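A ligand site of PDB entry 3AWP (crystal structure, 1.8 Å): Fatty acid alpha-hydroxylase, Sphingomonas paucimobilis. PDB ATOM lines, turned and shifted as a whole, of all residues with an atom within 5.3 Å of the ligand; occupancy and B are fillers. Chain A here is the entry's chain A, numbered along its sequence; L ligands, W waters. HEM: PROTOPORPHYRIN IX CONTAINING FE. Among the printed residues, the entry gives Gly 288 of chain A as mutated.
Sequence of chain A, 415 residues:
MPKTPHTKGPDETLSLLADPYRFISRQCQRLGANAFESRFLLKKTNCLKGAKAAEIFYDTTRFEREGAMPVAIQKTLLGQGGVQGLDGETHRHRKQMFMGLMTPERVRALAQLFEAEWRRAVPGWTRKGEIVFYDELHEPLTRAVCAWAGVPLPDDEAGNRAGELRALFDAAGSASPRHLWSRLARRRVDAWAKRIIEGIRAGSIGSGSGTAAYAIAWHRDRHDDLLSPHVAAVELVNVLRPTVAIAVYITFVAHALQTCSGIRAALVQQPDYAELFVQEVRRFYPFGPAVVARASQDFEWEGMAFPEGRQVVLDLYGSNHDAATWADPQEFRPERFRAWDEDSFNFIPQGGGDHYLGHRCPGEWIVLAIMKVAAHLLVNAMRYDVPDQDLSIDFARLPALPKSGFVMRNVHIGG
NH1 of Arg 65 lies within salt-bridge range of O2A of the ligand.
O1D of the ligand sits at hydrogen-bond distance from NE2 of His 91.
An oxygen (O2D) of the ligand lies within hydrogen-bond range of a ring nitrogen (ND1) of His 359.
SG of Cys 361 binds FE of the ligand (2.3 Å).
The side-chain hydroxyl of Tyr 58 lies within hydrogen-bond range of an oxygen (O1A) of the ligand, 2.6 Å away.
NZ of Lys 95 lies within salt-bridge range of O1D of the ligand (2.8 Å).
Water W5 lies within hydrogen-bond range of the side-chain amide oxygen (OD1) of Asn 238 (3.1 Å) and the side-chain amide nitrogen (NE2) of Gln 84 (3.2 Å).
The backbone NH (N) of Gly 363 sits close to the side-chain sulfur (SG) of Cys 361.
The backbone carbonyl oxygen (O) of Val 239 lies within hydrogen-bond range of the side-chain hydroxyl (OG1) of Thr 243 (2.8 Å).
The side-chain amide oxygen (OD1) of Asn 238 sits at hydrogen-bond distance from the side-chain amide nitrogen (NE2) of Gln 84 (3.3 Å).
A ring nitrogen (ND1) of His 359 lies close to a ring nitrogen (NE2) of His 91 (3.3 Å).
The backbone carbonyl oxygen of Gly 358 lies within hydrogen-bond range of the side-chain amino group of Lys 95.
The backbone NH of Cys 361 is in hydrogen-bond range of the backbone carbonyl oxygen of Gln 350.
The side-chain amino group (NZ) of Lys 95 is in hydrogen-bond range of the backbone carbonyl oxygen (O) of Arg 360 (2.7 Å).
OH of Tyr 58 sits at hydrogen-bond distance from N of Gly 352.
The side-chain amide nitrogen (NE2) of Gln 350 sits close to a nitrogen (NB) of the ligand (3.3 Å).
Merely in contact with the ligand: Val 83 (3.7 Å), Gln 84 (3.5 Å), Phe 98 (3.7 Å), Asn 238 (3.5 Å), Val 239 (3.8 Å), Pro 242 (3.3 Å), Thr 243 (3.5 Å), Ala 245 (3.6 Å), Ile 246 (3.6 Å), Tyr 249 (3.8 Å), Phe 287 (3.4 Å), Val 291 (3.5 Å), Leu 316 (3.4 Å), Gly 351 (3.9 Å), Gly 358 (3.9 Å), Pro 362 (3.4 Å), Gly 363 (3.5 Å), Ile 366 (3.5 Å) and Val 367 (3.6 Å).
26 residues have an atom within 4 Å of the ligand: Tyr 58, Arg 65, Val 83, Gln 84, His 91, Lys 95, Phe 98, Asn 238, Val 239, Pro 242, Thr 243, Ala 245, Ile 246, Tyr 249, Phe 287, Val 291, Leu 316, Gln 350, Gly 351, Gly 358, His 359, Cys 361, Pro 362, Gly 363, Ile 366 and Val 367.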
ATOM      1  N   PHE A  57      33.702  -3.315  16.436  1.00  0.00           N
ATOM      2  CA  PHE A  57      32.493  -2.567  16.063  1.00  0.00           C
ATOM      3  C   PHE A  57      32.730  -1.667  14.848  1.00  0.00           C
ATOM      4  O   PHE A  57      31.840  -1.489  13.989  1.00  0.00           O
ATOM      5  CB  PHE A  57      32.003  -1.743  17.258  1.00  0.00           C
ATOM      6  CG  PHE A  57      30.637  -1.118  17.073  1.00  0.00           C
ATOM      7  CD1 PHE A  57      29.474  -1.860  17.276  1.00  0.00           C
ATOM      8  CD2 PHE A  57      30.526   0.224  16.685  1.00  0.00           C
ATOM      9  CE1 PHE A  57      28.213  -1.266  17.116  1.00  0.00           C
ATOM     10  CE2 PHE A  57      29.265   0.832  16.528  1.00  0.00           C
ATOM     11  CZ  PHE A  57      28.112   0.076  16.726  1.00  0.00           C
ATOM     12  N   TYR A  58      33.945  -1.109  14.777  1.00  0.00           N
ATOM     13  CA  TYR A  58      34.335  -0.266  13.650  1.00  0.00           C
ATOM     14  C   TYR A  58      34.921  -0.999  12.447  1.00  0.00           C
ATOM     15  O   TYR A  58      35.315  -0.380  11.456  1.00  0.00           O
ATOM     16  CB  TYR A  58      35.235   0.895  14.114  1.00  0.00           C
ATOM     17  CG  TYR A  58      34.385   1.926  14.826  1.00  0.00           C
ATOM     18  CD1 TYR A  58      33.585   2.804  14.085  1.00  0.00           C
ATOM     19  CD2 TYR A  58      34.304   1.953  16.219  1.00  0.00           C
ATOM     20  CE1 TYR A  58      32.753   3.733  14.730  1.00  0.00           C
ATOM     21  CE2 TYR A  58      33.482   2.874  16.869  1.00  0.00           C
ATOM     22  CZ  TYR A  58      32.711   3.756  16.112  1.00  0.00           C
ATOM     23  OH  TYR A  58      31.919   4.673  16.750  1.00  0.00           O
ATOM     24  N   ARG A  65      25.538  -0.140   9.026  1.00  0.00           N
ATOM     25  CA  ARG A  65      24.571   0.717   9.693  1.00  0.00           C
ATOM     26  C   ARG A  65      23.247   0.763   8.964  1.00  0.00           C
ATOM     27  O   ARG A  65      22.250   1.207   9.557  1.00  0.00           O
ATOM     28  CB  ARG A  65      25.103   2.153   9.833  1.00  0.00           C
ATOM     29  CG  ARG A  65      26.504   2.233  10.485  1.00  0.00           C
ATOM     30  CD  ARG A  65      26.546   1.535  11.870  1.00  0.00           C
ATOM     31  NE  ARG A  65      27.841   1.755  12.533  1.00  0.00           N
ATOM     32  CZ  ARG A  65      28.179   2.862  13.194  1.00  0.00           C
ATOM     33  NH1 ARG A  65      27.309   3.871  13.308  1.00  0.00           N
ATOM     34  NH2 ARG A  65      29.387   2.973  13.743  1.00  0.00           N
ATOM     35  N   VAL A  83      23.780  10.717   6.620  1.00  0.00           N
ATOM     36  CA  VAL A  83      25.023   9.952   6.522  1.00  0.00           C
ATOM     37  C   VAL A  83      25.067   8.791   7.528  1.00  0.00           C
ATOM     38  O   VAL A  83      25.691   7.758   7.255  1.00  0.00           O
ATOM     39  CB  VAL A  83      26.243  10.936   6.696  1.00  0.00           C
ATOM     40  CG1 VAL A  83      26.254  11.619   8.105  1.00  0.00           C
ATOM     41  CG2 VAL A  83      27.573  10.215   6.394  1.00  0.00           C
ATOM     42  N   GLN A  84      24.392   8.935   8.671  1.00  0.00           N
ATOM     43  CA  GLN A  84      24.426   7.881   9.715  1.00  0.00           C
ATOM     44  C   GLN A  84      23.873   6.547   9.220  1.00  0.00           C
ATOM     45  O   GLN A  84      24.226   5.507   9.752  1.00  0.00           O
ATOM     46  CB  GLN A  84      23.639   8.303  10.970  1.00  0.00           C
ATOM     47  CG  GLN A  84      24.206   9.544  11.669  1.00  0.00           C
ATOM     48  CD  GLN A  84      23.623  10.841  11.164  1.00  0.00           C
ATOM     49  OE1 GLN A  84      22.961  10.889  10.122  1.00  0.00           O
ATOM     50  NE2 GLN A  84      23.859  11.923  11.896  1.00  0.00           N
ATOM     51  N   HIS A  91      28.652   5.716   1.811  1.00  0.00           N
ATOM     52  CA  HIS A  91      28.939   6.402   3.067  1.00  0.00           C
ATOM     53  C   HIS A  91      30.212   7.243   2.996  1.00  0.00           C
ATOM     54  O   HIS A  91      30.231   8.406   3.413  1.00  0.00           O
ATOM     55  CB  HIS A  91      29.093   5.419   4.236  1.00  0.00           C
ATOM     56  CG  HIS A  91      29.599   6.102   5.466  1.00  0.00           C
ATOM     57  ND1 HIS A  91      30.921   6.044   5.866  1.00  0.00           N
ATOM     58  CD2 HIS A  91      28.976   6.938   6.338  1.00  0.00           C
ATOM     59  CE1 HIS A  91      31.077   6.792   6.946  1.00  0.00           C
ATOM     60  NE2 HIS A  91      29.907   7.326   7.265  1.00  0.00           N
ATOM     61  N   LYS A  95      30.499  11.112   3.704  1.00  0.00           N
ATOM     62  CA  LYS A  95      31.257  11.503   4.905  1.00  0.00           C
ATOM     63  C   LYS A  95      32.330  12.556   4.551  1.00  0.00           C
ATOM     64  O   LYS A  95      32.575  13.497   5.305  1.00  0.00           O
ATOM     65  CB  LYS A  95      31.884  10.268   5.571  1.00  0.00           C
ATOM     66  CG  LYS A  95      32.678  10.566   6.879  1.00  0.00           C
ATOM     67  CD  LYS A  95      31.808  11.368   7.887  1.00  0.00           C
ATOM     68  CE  LYS A  95      32.429  11.318   9.318  1.00  0.00           C
ATOM     69  NZ  LYS A  95      32.391   9.918   9.900  1.00  0.00           N
ATOM     70  N   PHE A  98      31.171  16.153   4.871  1.00  0.00           N
ATOM     71  CA  PHE A  98      31.252  16.734   6.222  1.00  0.00           C
ATOM     72  C   PHE A  98      32.687  17.034   6.618  1.00  0.00           C
ATOM     73  O   PHE A  98      32.980  18.084   7.199  1.00  0.00           O
ATOM     74  CB  PHE A  98      30.656  15.769   7.253  1.00  0.00           C
ATOM     75  CG  PHE A  98      29.146  15.710   7.219  1.00  0.00           C
ATOM     76  CD1 PHE A  98      28.387  16.656   7.896  1.00  0.00           C
ATOM     77  CD2 PHE A  98      28.497  14.692   6.510  1.00  0.00           C
ATOM     78  CE1 PHE A  98      26.996  16.635   7.865  1.00  0.00           C
ATOM     79  CE2 PHE A  98      27.058  14.628   6.475  1.00  0.00           C
ATOM     80  CZ  PHE A  98      26.317  15.602   7.156  1.00  0.00           C
ATOM     81  N   MET A 102      35.777  20.911   7.975  1.00  0.00           N
ATOM     82  CA  MET A 102      36.420  20.979   9.290  1.00  0.00           C
ATOM     83  C   MET A 102      37.888  21.423   9.276  1.00  0.00           C
ATOM     84  O   MET A 102      38.697  20.981  10.112  1.00  0.00           O
ATOM     85  CB  MET A 102      36.302  19.619   9.983  1.00  0.00           C
ATOM     86  CG  MET A 102      34.871  19.091  10.027  1.00  0.00           C
ATOM     87  SD  MET A 102      33.717  20.322  10.711  1.00  0.00           S
ATOM     88  CE  MET A 102      32.208  19.355  10.667  1.00  0.00           C
ATOM     89  N   ASN A 238      22.208  18.011  10.275  1.00  0.00           N
ATOM     90  CA  ASN A 238      23.305  17.253  10.928  1.00  0.00           C
ATOM     91  C   ASN A 238      24.567  18.084  11.248  1.00  0.00           C
ATOM     92  O   ASN A 238      25.481  17.576  11.892  1.00  0.00           O
ATOM     93  CB  ASN A 238      23.686  16.025  10.068  1.00  0.00           C
ATOM     94  CG  ASN A 238      22.734  14.861  10.270  1.00  0.00           C
ATOM     95  OD1 ASN A 238      22.189  14.673  11.359  1.00  0.00           O
ATOM     96  ND2 ASN A 238      22.554  14.053   9.232  1.00  0.00           N
ATOM     97  N   VAL A 239      24.622  19.335  10.764  1.00  0.00           N
ATOM     98  CA  VAL A 239      25.648  20.296  11.196  1.00  0.00           C
ATOM     99  C   VAL A 239      25.060  21.217  12.262  1.00  0.00           C
ATOM    100  O   VAL A 239      25.671  21.425  13.318  1.00  0.00           O
ATOM    101  CB  VAL A 239      26.151  21.156  10.001  1.00  0.00           C
ATOM    102  CG1 VAL A 239      27.187  22.237  10.485  1.00  0.00           C
ATOM    103  CG2 VAL A 239      26.779  20.237   8.931  1.00  0.00           C
ATOM    104  N   PRO A 242      23.745  19.223  16.044  1.00  0.00           N
ATOM    105  CA  PRO A 242      24.751  18.797  17.036  1.00  0.00           C
ATOM    106  C   PRO A 242      25.635  19.949  17.544  1.00  0.00           C
ATOM    107  O   PRO A 242      26.182  19.873  18.636  1.00  0.00           O
ATOM    108  CB  PRO A 242      25.596  17.769  16.275  1.00  0.00           C
ATOM    109  CG  PRO A 242      24.911  17.537  14.975  1.00  0.00           C
ATOM    110  CD  PRO A 242      23.977  18.647  14.703  1.00  0.00           C
ATOM    111  N   THR A 243      25.787  21.006  16.748  1.00  0.00           N
ATOM    112  CA  THR A 243      26.519  22.190  17.257  1.00  0.00           C
ATOM    113  C   THR A 243      25.753  22.826  18.417  1.00  0.00           C
ATOM    114  O   THR A 243      26.354  23.211  19.452  1.00  0.00           O
ATOM    115  CB  THR A 243      26.832  23.195  16.136  1.00  0.00           C
ATOM    116  OG1 THR A 243      27.572  22.526  15.097  1.00  0.00           O
ATOM    117  CG2 THR A 243      27.655  24.394  16.653  1.00  0.00           C
ATOM    118  N   ALA A 245      23.801  21.138  20.335  1.00  0.00           N
ATOM    119  CA  ALA A 245      23.947  20.150  21.424  1.00  0.00           C
ATOM    120  C   ALA A 245      25.221  20.348  22.260  1.00  0.00           C
ATOM    121  O   ALA A 245      25.308  19.802  23.372  1.00  0.00           O
ATOM    122  CB  ALA A 245      23.888  18.708  20.882  1.00  0.00           C
ATOM    123  N   ILE A 246      26.161  21.158  21.776  1.00  0.00           N
ATOM    124  CA  ILE A 246      27.355  21.502  22.593  1.00  0.00           C
ATOM    125  C   ILE A 246      26.952  22.231  23.904  1.00  0.00           C
ATOM    126  O   ILE A 246      27.707  22.186  24.878  1.00  0.00           O
ATOM    127  CB  ILE A 246      28.454  22.263  21.769  1.00  0.00           C
ATOM    128  CG1 ILE A 246      28.864  21.397  20.560  1.00  0.00           C
ATOM    129  CG2 ILE A 246      29.686  22.581  22.649  1.00  0.00           C
ATOM    130  CD1 ILE A 246      29.698  22.143  19.501  1.00  0.00           C
ATOM    131  N   TYR A 249      27.720  19.892  26.746  1.00  0.00           N
ATOM    132  CA  TYR A 249      29.131  19.910  27.174  1.00  0.00           C
ATOM    133  C   TYR A 249      29.556  21.198  27.876  1.00  0.00           C
ATOM    134  O   TYR A 249      30.360  21.144  28.829  1.00  0.00           O
ATOM    135  CB  TYR A 249      30.078  19.660  25.986  1.00  0.00           C
ATOM    136  CG  TYR A 249      30.398  18.202  25.704  1.00  0.00           C
ATOM    137  CD1 TYR A 249      30.616  17.285  26.741  1.00  0.00           C
ATOM    138  CD2 TYR A 249      30.536  17.750  24.383  1.00  0.00           C
ATOM    139  CE1 TYR A 249      30.932  15.941  26.467  1.00  0.00           C
ATOM    140  CE2 TYR A 249      30.869  16.404  24.086  1.00  0.00           C
ATOM    141  CZ  TYR A 249      31.058  15.510  25.145  1.00  0.00           C
ATOM    142  OH  TYR A 249      31.372  14.182  24.861  1.00  0.00           O
ATOM    143  N   PHE A 287      27.194  11.493  27.686  1.00  0.00           N
ATOM    144  CA  PHE A 287      26.503  12.336  26.708  1.00  0.00           C
ATOM    145  C   PHE A 287      26.063  11.453  25.546  1.00  0.00           C
ATOM    146  O   PHE A 287      24.854  11.242  25.339  1.00  0.00           O
ATOM    147  CB  PHE A 287      27.431  13.492  26.261  1.00  0.00           C
ATOM    148  CG  PHE A 287      26.746  14.586  25.464  1.00  0.00           C
ATOM    149  CD1 PHE A 287      25.421  14.480  25.052  1.00  0.00           C
ATOM    150  CD2 PHE A 287      27.480  15.730  25.086  1.00  0.00           C
ATOM    151  CE1 PHE A 287      24.815  15.508  24.306  1.00  0.00           C
ATOM    152  CE2 PHE A 287      26.893  16.748  24.322  1.00  0.00           C
ATOM    153  CZ  PHE A 287      25.550  16.643  23.934  1.00  0.00           C
ATOM    154  N   GLY A 288      27.004  10.935  24.776  1.00  0.00           N
ATOM    155  CA  GLY A 288      26.635  10.100  23.637  1.00  0.00           C
ATOM    156  C   GLY A 288      26.070   8.775  24.111  1.00  0.00           C
ATOM    157  O   GLY A 288      26.743   8.063  24.871  1.00  0.00           O
ATOM    158  N   PRO A 289      24.845   8.415  23.680  1.00  0.00           N
ATOM    159  CA  PRO A 289      24.306   7.116  24.026  1.00  0.00           C
ATOM    160  C   PRO A 289      24.996   6.040  23.200  1.00  0.00           C
ATOM    161  O   PRO A 289      25.763   6.365  22.281  1.00  0.00           O
ATOM    162  CB  PRO A 289      22.822   7.238  23.642  1.00  0.00           C
ATOM    163  CG  PRO A 289      22.585   8.748  23.476  1.00  0.00           C
ATOM    164  CD  PRO A 289      23.875   9.207  22.912  1.00  0.00           C
ATOM    165  N   VAL A 291      25.984   3.419  20.456  1.00  0.00           N
ATOM    166  CA  VAL A 291      25.845   3.449  19.004  1.00  0.00           C
ATOM    167  C   VAL A 291      25.346   2.089  18.534  1.00  0.00           C
ATOM    168  O   VAL A 291      25.752   1.073  19.094  1.00  0.00           O
ATOM    169  CB  VAL A 291      27.201   3.760  18.329  1.00  0.00           C
ATOM    170  CG1 VAL A 291      27.076   3.722  16.788  1.00  0.00           C
ATOM    171  CG2 VAL A 291      27.709   5.120  18.797  1.00  0.00           C
ATOM    172  N   LEU A 316      29.578   3.744  24.683  1.00  0.00           N
ATOM    173  CA  LEU A 316      30.630   4.777  24.704  1.00  0.00           C
ATOM    174  C   LEU A 316      31.020   5.161  26.141  1.00  0.00           C
ATOM    175  O   LEU A 316      32.212   5.190  26.493  1.00  0.00           O
ATOM    176  CB  LEU A 316      30.173   6.023  23.935  1.00  0.00           C
ATOM    177  CG  LEU A 316      29.667   5.765  22.508  1.00  0.00           C
ATOM    178  CD1 LEU A 316      29.247   7.111  21.850  1.00  0.00           C
ATOM    179  CD2 LEU A 316      30.723   5.011  21.671  1.00  0.00           C
ATOM    180  N   PRO A 349      34.130   9.339  23.187  1.00  0.00           N
ATOM    181  CA  PRO A 349      32.918  10.075  23.566  1.00  0.00           C
ATOM    182  C   PRO A 349      32.051  10.460  22.340  1.00  0.00           C
ATOM    183  O   PRO A 349      30.850  10.652  22.491  1.00  0.00           O
ATOM    184  CB  PRO A 349      33.450  11.352  24.233  1.00  0.00           C
ATOM    185  CG  PRO A 349      34.828  11.549  23.619  1.00  0.00           C
ATOM    186  CD  PRO A 349      35.362  10.137  23.387  1.00  0.00           C
ATOM    187  N   GLN A 350      32.682  10.553  21.164  1.00  0.00           N
ATOM    188  CA  GLN A 350      31.948  10.844  19.918  1.00  0.00           C
ATOM    189  C   GLN A 350      32.282   9.779  18.857  1.00  0.00           C
ATOM    190  O   GLN A 350      32.398  10.065  17.661  1.00  0.00           O
ATOM    191  CB  GLN A 350      32.288  12.284  19.456  1.00  0.00           C
ATOM    192  CG  GLN A 350      31.908  13.327  20.546  1.00  0.00           C
ATOM    193  CD  GLN A 350      32.239  14.766  20.194  1.00  0.00           C
ATOM    194  OE1 GLN A 350      32.812  15.480  21.002  1.00  0.00           O
ATOM    195  NE2 GLN A 350      31.835  15.221  18.996  1.00  0.00           N
ATOM    196  N   GLY A 351      32.425   8.551  19.324  1.00  0.00           N
ATOM    197  CA  GLY A 351      32.721   7.431  18.459  1.00  0.00           C
ATOM    198  C   GLY A 351      34.204   7.107  18.351  1.00  0.00           C
ATOM    199  O   GLY A 351      35.052   7.869  18.820  1.00  0.00           O
ATOM    200  N   GLY A 352      34.496   5.970  17.738  1.00  0.00           N
ATOM    201  CA  GLY A 352      35.874   5.466  17.613  1.00  0.00           C
ATOM    202  C   GLY A 352      36.248   5.278  16.161  1.00  0.00           C
ATOM    203  O   GLY A 352      35.468   5.564  15.246  1.00  0.00           O
ATOM    204  N   GLY A 358      34.885   5.452   8.572  1.00  0.00           N
ATOM    205  CA  GLY A 358      33.895   4.947   9.494  1.00  0.00           C
ATOM    206  C   GLY A 358      32.960   6.068   9.899  1.00  0.00           C
ATOM    207  O   GLY A 358      33.088   7.174   9.385  1.00  0.00           O
ATOM    208  N   HIS A 359      32.061   5.787  10.835  1.00  0.00           N
ATOM    209  CA  HIS A 359      31.032   6.740  11.238  1.00  0.00           C
ATOM    210  C   HIS A 359      31.418   7.695  12.392  1.00  0.00           C
ATOM    211  O   HIS A 359      30.571   8.427  12.905  1.00  0.00           O
ATOM    212  CB  HIS A 359      29.767   5.975  11.607  1.00  0.00           C
ATOM    213  CG  HIS A 359      29.067   5.425  10.411  1.00  0.00           C
ATOM    214  ND1 HIS A 359      28.063   6.121   9.757  1.00  0.00           N
ATOM    215  CD2 HIS A 359      29.268   4.290   9.706  1.00  0.00           C
ATOM    216  CE1 HIS A 359      27.658   5.408   8.720  1.00  0.00           C
ATOM    217  NE2 HIS A 359      28.368   4.294   8.674  1.00  0.00           N
ATOM    218  N   ARG A 360      32.685   7.682  12.779  1.00  0.00           N
ATOM    219  CA  ARG A 360      33.146   8.569  13.853  1.00  0.00           C
ATOM    220  C   ARG A 360      32.705  10.014  13.624  1.00  0.00           C
ATOM    221  O   ARG A 360      32.746  10.533  12.484  1.00  0.00           O
ATOM    222  CB  ARG A 360      34.690   8.504  13.966  1.00  0.00           C
ATOM    223  CG  ARG A 360      35.219   9.288  15.164  1.00  0.00           C
ATOM    224  CD  ARG A 360      36.762   9.053  15.293  1.00  0.00           C
ATOM    225  NE  ARG A 360      37.216   9.744  16.509  1.00  0.00           N
ATOM    226  CZ  ARG A 360      37.980   9.194  17.444  1.00  0.00           C
ATOM    227  NH1 ARG A 360      38.473   7.962  17.276  1.00  0.00           N
ATOM    228  NH2 ARG A 360      38.300   9.902  18.526  1.00  0.00           N
ATOM    229  N   CYS A 361      32.292  10.667  14.711  1.00  0.00           N
ATOM    230  CA  CYS A 361      31.797  12.067  14.624  1.00  0.00           C
ATOM    231  C   CYS A 361      32.792  13.044  13.965  1.00  0.00           C
ATOM    232  O   CYS A 361      33.920  13.211  14.447  1.00  0.00           O
ATOM    233  CB  CYS A 361      31.495  12.575  16.039  1.00  0.00           C
ATOM    234  SG  CYS A 361      30.819  14.227  16.074  1.00  0.00           S
ATOM    235  N   PRO A 362      32.359  13.733  12.891  1.00  0.00           N
ATOM    236  CA  PRO A 362      33.215  14.737  12.261  1.00  0.00           C
ATOM    237  C   PRO A 362      33.213  16.058  13.032  1.00  0.00           C
ATOM    238  O   PRO A 362      33.992  16.965  12.688  1.00  0.00           O
ATOM    239  CB  PRO A 362      32.562  14.916  10.867  1.00  0.00           C
ATOM    240  CG  PRO A 362      31.071  14.719  11.152  1.00  0.00           C
ATOM    241  CD  PRO A 362      31.048  13.604  12.204  1.00  0.00           C
ATOM    242  N   GLY A 363      32.346  16.158  14.049  1.00  0.00           N
ATOM    243  CA  GLY A 363      32.186  17.383  14.811  1.00  0.00           C
ATOM    244  C   GLY A 363      33.190  17.547  15.952  1.00  0.00           C
ATOM    245  O   GLY A 363      33.120  18.532  16.699  1.00  0.00           O
ATOM    246  N   ILE A 366      35.168  20.941  16.158  1.00  0.00           N
ATOM    247  CA  ILE A 366      34.259  21.985  16.589  1.00  0.00           C
ATOM    248  C   ILE A 366      33.952  21.898  18.086  1.00  0.00           C
ATOM    249  O   ILE A 366      33.988  22.922  18.800  1.00  0.00           O
ATOM    250  CB  ILE A 366      32.951  21.946  15.782  1.00  0.00           C
ATOM    251  CG1 ILE A 366      33.217  22.408  14.352  1.00  0.00           C
ATOM    252  CG2 ILE A 366      31.881  22.851  16.449  1.00  0.00           C
ATOM    253  CD1 ILE A 366      32.053  22.108  13.360  1.00  0.00           C
ATOM    254  N   VAL A 367      33.601  20.696  18.547  1.00  0.00           N
ATOM    255  CA  VAL A 367      33.291  20.491  19.955  1.00  0.00           C
ATOM    256  C   VAL A 367      34.476  20.940  20.823  1.00  0.00           C
ATOM    257  O   VAL A 367      34.288  21.701  21.798  1.00  0.00           O
ATOM    258  CB  VAL A 367      32.898  19.007  20.269  1.00  0.00           C
ATOM    259  CG1 VAL A 367      32.834  18.754  21.800  1.00  0.00           C
ATOM    260  CG2 VAL A 367      31.523  18.686  19.666  1.00  0.00           C
HETATM  261  CHA HEM L   1      28.276  11.117  14.603  1.00  0.00           C
HETATM  262  CHB HEM L   1      28.608  12.273  19.281  1.00  0.00           C
HETATM  263  CHC HEM L   1      28.852  16.955  18.048  1.00  0.00           C
HETATM  264  CHD HEM L   1      28.151  15.838  13.418  1.00  0.00           C
HETATM  265  C1A HEM L   1      28.388  11.034  15.960  1.00  0.00           C
HETATM  266  C2A HEM L   1      28.399   9.804  16.702  1.00  0.00           C
HETATM  267  C3A HEM L   1      28.507  10.121  18.010  1.00  0.00           C
HETATM  268  C4A HEM L   1      28.542  11.560  18.112  1.00  0.00           C
HETATM  269  CMA HEM L   1      28.532   9.132  19.192  1.00  0.00           C
HETATM  270  CAA HEM L   1      28.259   8.412  16.084  1.00  0.00           C
HETATM  271  CBA HEM L   1      29.549   7.644  15.864  1.00  0.00           C
HETATM  272  CGA HEM L   1      29.192   6.357  15.132  1.00  0.00           C
HETATM  273  O1A HEM L   1      30.039   5.426  15.123  1.00  0.00           O
HETATM  274  O2A HEM L   1      28.063   6.224  14.555  1.00  0.00           O
HETATM  275  C1B HEM L   1      28.563  13.650  19.357  1.00  0.00           C
HETATM  276  C2B HEM L   1      28.450  14.421  20.573  1.00  0.00           C
HETATM  277  C3B HEM L   1      28.508  15.725  20.245  1.00  0.00           C
HETATM  278  C4B HEM L   1      28.668  15.813  18.793  1.00  0.00           C
HETATM  279  CMB HEM L   1      28.278  13.836  21.982  1.00  0.00           C
HETATM  280  CAB HEM L   1      28.394  16.890  21.236  1.00  0.00           C
HETATM  281  CBB HEM L   1      27.664  18.000  20.985  1.00  0.00           C
HETATM  282  C1C HEM L   1      28.809  17.064  16.681  1.00  0.00           C
HETATM  283  C2C HEM L   1      28.967  18.268  15.908  1.00  0.00           C
HETATM  284  C3C HEM L   1      28.759  17.947  14.610  1.00  0.00           C
HETATM  285  C4C HEM L   1      28.457  16.540  14.566  1.00  0.00           C
HETATM  286  CMC HEM L   1      29.307  19.653  16.516  1.00  0.00           C
HETATM  287  CAC HEM L   1      28.790  18.800  13.321  1.00  0.00           C
HETATM  288  CBC HEM L   1      29.242  20.047  13.279  1.00  0.00           C
HETATM  289  C1D HEM L   1      28.014  14.472  13.336  1.00  0.00           C
HETATM  290  C2D HEM L   1      27.691  13.770  12.117  1.00  0.00           C
HETATM  291  C3D HEM L   1      27.745  12.315  12.489  1.00  0.00           C
HETATM  292  C4D HEM L   1      28.110  12.273  13.885  1.00  0.00           C
HETATM  293  CMD HEM L   1      27.352  14.380  10.740  1.00  0.00           C
HETATM  294  CAD HEM L   1      27.493  11.109  11.551  1.00  0.00           C
HETATM  295  CBD HEM L   1      28.891  10.721  10.976  1.00  0.00           C
HETATM  296  CGD HEM L   1      28.788   9.440  10.174  1.00  0.00           C
HETATM  297  O1D HEM L   1      29.732   9.075   9.399  1.00  0.00           O
HETATM  298  O2D HEM L   1      27.737   8.756  10.317  1.00  0.00           O
HETATM  299  NA  HEM L   1      28.468  12.097  16.836  1.00  0.00           N
HETATM  300  NB  HEM L   1      28.687  14.522  18.302  1.00  0.00           N
HETATM  301  NC  HEM L   1      28.520  16.011  15.837  1.00  0.00           N
HETATM  302  ND  HEM L   1      28.259  13.573  14.359  1.00  0.00           N
HETATM  303 FE   HEM L   1      28.528  14.047  16.321  1.00  0.00          FE
HETATM  304  O   HOH W   1      24.979  11.938  14.606  1.00  0.00           O
HETATM  305  O   HOH W   2      26.526   7.626  12.834  1.00  0.00           O
HETATM  306  O   HOH W   3      25.125   6.570  14.908  1.00  0.00           O
HETATM  307  O   HOH W   4      26.350  14.145  16.423  1.00  0.00           O
HETATM  308  O   HOH W   5      24.752  14.716  13.131  1.00  0.00           O
